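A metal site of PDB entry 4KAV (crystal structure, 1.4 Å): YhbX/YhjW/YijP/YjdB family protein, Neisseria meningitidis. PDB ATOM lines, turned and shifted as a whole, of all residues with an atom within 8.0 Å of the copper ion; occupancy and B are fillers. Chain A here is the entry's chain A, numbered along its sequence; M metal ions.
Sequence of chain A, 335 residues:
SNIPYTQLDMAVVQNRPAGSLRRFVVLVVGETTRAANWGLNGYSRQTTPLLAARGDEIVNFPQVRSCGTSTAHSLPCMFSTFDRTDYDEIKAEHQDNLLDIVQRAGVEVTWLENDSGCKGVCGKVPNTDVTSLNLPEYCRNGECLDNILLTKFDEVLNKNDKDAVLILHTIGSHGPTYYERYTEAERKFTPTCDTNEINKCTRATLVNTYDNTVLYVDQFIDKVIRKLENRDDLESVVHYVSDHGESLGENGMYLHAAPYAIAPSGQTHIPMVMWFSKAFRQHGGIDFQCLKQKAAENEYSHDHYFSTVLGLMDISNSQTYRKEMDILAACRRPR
A ring nitrogen (ND1) of His 94 lies within hydrogen-bond range of the backbone carbonyl oxygen (O) of Ile 90, 2.7 Å away.
Within 4 Å of the copper ion: Ser 1, Asn 2 and His 94.
The nearest printed residue that does not touch the copper ion is Ile 3 (4.03 Å).
The copper ion is bound by NE2 of His 94 (2.1 Å), N of Ser 1 (2.2 Å) and N of Asn 2 (2.2 Å).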
ATOM      1  N   SER A   1     -12.494  -5.938  -0.496  1.00  0.00           N
ATOM      2  CA  SER A   1     -13.833  -5.474  -0.174  1.00  0.00           C
ATOM      3  C   SER A   1     -14.722  -5.322  -1.403  1.00  0.00           C
ATOM      4  O   SER A   1     -15.930  -5.128  -1.278  1.00  0.00           O
ATOM      5  CB  SER A   1     -13.750  -4.115   0.527  1.00  0.00           C
ATOM      6  OG  SER A   1     -14.355  -4.186   1.808  1.00  0.00           O
ATOM      7  N   ASN A   2     -14.146  -5.398  -2.601  1.00  0.00           N
ATOM      8  CA  ASN A   2     -14.834  -5.135  -3.875  1.00  0.00           C
ATOM      9  C   ASN A   2     -15.992  -6.087  -4.138  1.00  0.00           C
ATOM     10  O   ASN A   2     -16.918  -5.794  -4.902  1.00  0.00           O
ATOM     11  CB  ASN A   2     -13.826  -5.262  -5.020  1.00  0.00           C
ATOM     12  CG  ASN A   2     -14.446  -5.005  -6.392  1.00  0.00           C
ATOM     13  OD1 ASN A   2     -15.066  -3.975  -6.628  1.00  0.00           O
ATOM     14  ND2 ASN A   2     -14.279  -5.960  -7.301  1.00  0.00           N
ATOM     15  N   ILE A   3     -15.866  -7.284  -3.585  1.00  0.00           N
ATOM     16  CA  ILE A   3     -16.925  -8.273  -3.701  1.00  0.00           C
ATOM     17  C   ILE A   3     -16.980  -8.959  -2.348  1.00  0.00           C
ATOM     18  O   ILE A   3     -15.993  -8.991  -1.623  1.00  0.00           O
ATOM     19  CB  ILE A   3     -16.682  -9.272  -4.846  1.00  0.00           C
ATOM     20  CG1 ILE A   3     -15.498 -10.180  -4.526  1.00  0.00           C
ATOM     21  CG2 ILE A   3     -16.441  -8.522  -6.163  1.00  0.00           C
ATOM     22  CD1 ILE A   3     -15.239 -11.243  -5.593  1.00  0.00           C
ATOM     23  N   PRO A   4     -18.155  -9.493  -1.977  1.00  0.00           N
ATOM     24  CA  PRO A   4     -18.205 -10.108  -0.649  1.00  0.00           C
ATOM     25  C   PRO A   4     -17.195 -11.240  -0.514  1.00  0.00           C
ATOM     26  O   PRO A   4     -16.942 -11.967  -1.462  1.00  0.00           O
ATOM     27  CB  PRO A   4     -19.641 -10.638  -0.545  1.00  0.00           C
ATOM     28  CG  PRO A   4     -20.229 -10.506  -1.917  1.00  0.00           C
ATOM     29  CD  PRO A   4     -19.482  -9.434  -2.621  1.00  0.00           C
ATOM     30  N   TYR A   5     -16.618 -11.363   0.683  1.00  0.00           N
ATOM     31  CA  TYR A   5     -15.638 -12.389   0.942  1.00  0.00           C
ATOM     32  C   TYR A   5     -16.350 -13.690   1.262  1.00  0.00           C
ATOM     33  O   TYR A   5     -17.273 -13.727   2.072  1.00  0.00           O
ATOM     34  CB  TYR A   5     -14.734 -11.988   2.102  1.00  0.00           C
ATOM     35  CG  TYR A   5     -13.601 -12.948   2.373  1.00  0.00           C
ATOM     36  CD1 TYR A   5     -13.800 -14.070   3.172  1.00  0.00           C
ATOM     37  CD2 TYR A   5     -12.348 -12.729   1.849  1.00  0.00           C
ATOM     38  CE1 TYR A   5     -12.756 -14.954   3.426  1.00  0.00           C
ATOM     39  CE2 TYR A   5     -11.297 -13.620   2.094  1.00  0.00           C
ATOM     40  CZ  TYR A   5     -11.508 -14.715   2.895  1.00  0.00           C
ATOM     41  OH  TYR A   5     -10.468 -15.594   3.142  1.00  0.00           O
ATOM     42  N   ILE A  90      -9.467 -12.051  -8.924  1.00  0.00           N
ATOM     43  CA  ILE A  90     -10.306 -11.293  -7.983  1.00  0.00           C
ATOM     44  C   ILE A  90     -11.101 -12.230  -7.089  1.00  0.00           C
ATOM     45  O   ILE A  90     -11.195 -12.016  -5.866  1.00  0.00           O
ATOM     46  CB  ILE A  90     -11.285 -10.378  -8.733  1.00  0.00           C
ATOM     47  CG1 ILE A  90     -10.544  -9.565  -9.800  1.00  0.00           C
ATOM     48  CG2 ILE A  90     -11.977  -9.445  -7.752  1.00  0.00           C
ATOM     49  CD1 ILE A  90      -9.223  -8.974  -9.327  1.00  0.00           C
ATOM     50  N   GLU A  93      -8.829 -13.829  -4.528  1.00  0.00           N
ATOM     51  CA  GLU A  93      -8.394 -12.895  -3.496  1.00  0.00           C
ATOM     52  C   GLU A  93      -9.477 -12.655  -2.455  1.00  0.00           C
ATOM     53  O   GLU A  93      -9.198 -12.182  -1.359  1.00  0.00           O
ATOM     54  CB  GLU A  93      -7.969 -11.574  -4.144  1.00  0.00           C
ATOM     55  CG  GLU A  93      -7.693 -10.440  -3.167  1.00  0.00           C
ATOM     56  CD  GLU A  93      -6.412 -10.607  -2.368  1.00  0.00           C
ATOM     57  OE1 GLU A  93      -5.649 -11.597  -2.600  1.00  0.00           O
ATOM     58  OE2 GLU A  93      -6.165  -9.740  -1.503  1.00  0.00           O
ATOM     59  N   HIS A  94     -10.728 -12.959  -2.789  1.00  0.00           N
ATOM     60  CA  HIS A  94     -11.863 -12.644  -1.927  1.00  0.00           C
ATOM     61  C   HIS A  94     -12.518 -13.934  -1.424  1.00  0.00           C
ATOM     62  O   HIS A  94     -13.751 -13.978  -1.199  1.00  0.00           O
ATOM     63  CB  HIS A  94     -12.883 -11.790  -2.683  1.00  0.00           C
ATOM     64  CG  HIS A  94     -12.425 -10.391  -2.943  1.00  0.00           C
ATOM     65  ND1 HIS A  94     -11.647 -10.039  -4.028  1.00  0.00           N
ATOM     66  CD2 HIS A  94     -12.653  -9.244  -2.262  1.00  0.00           C
ATOM     67  CE1 HIS A  94     -11.403  -8.735  -3.993  1.00  0.00           C
ATOM     68  NE2 HIS A  94     -12.021  -8.225  -2.942  1.00  0.00           N
HETATM   69 CU    CU M   1     -12.121  -6.146  -2.605  1.00  0.00          CU
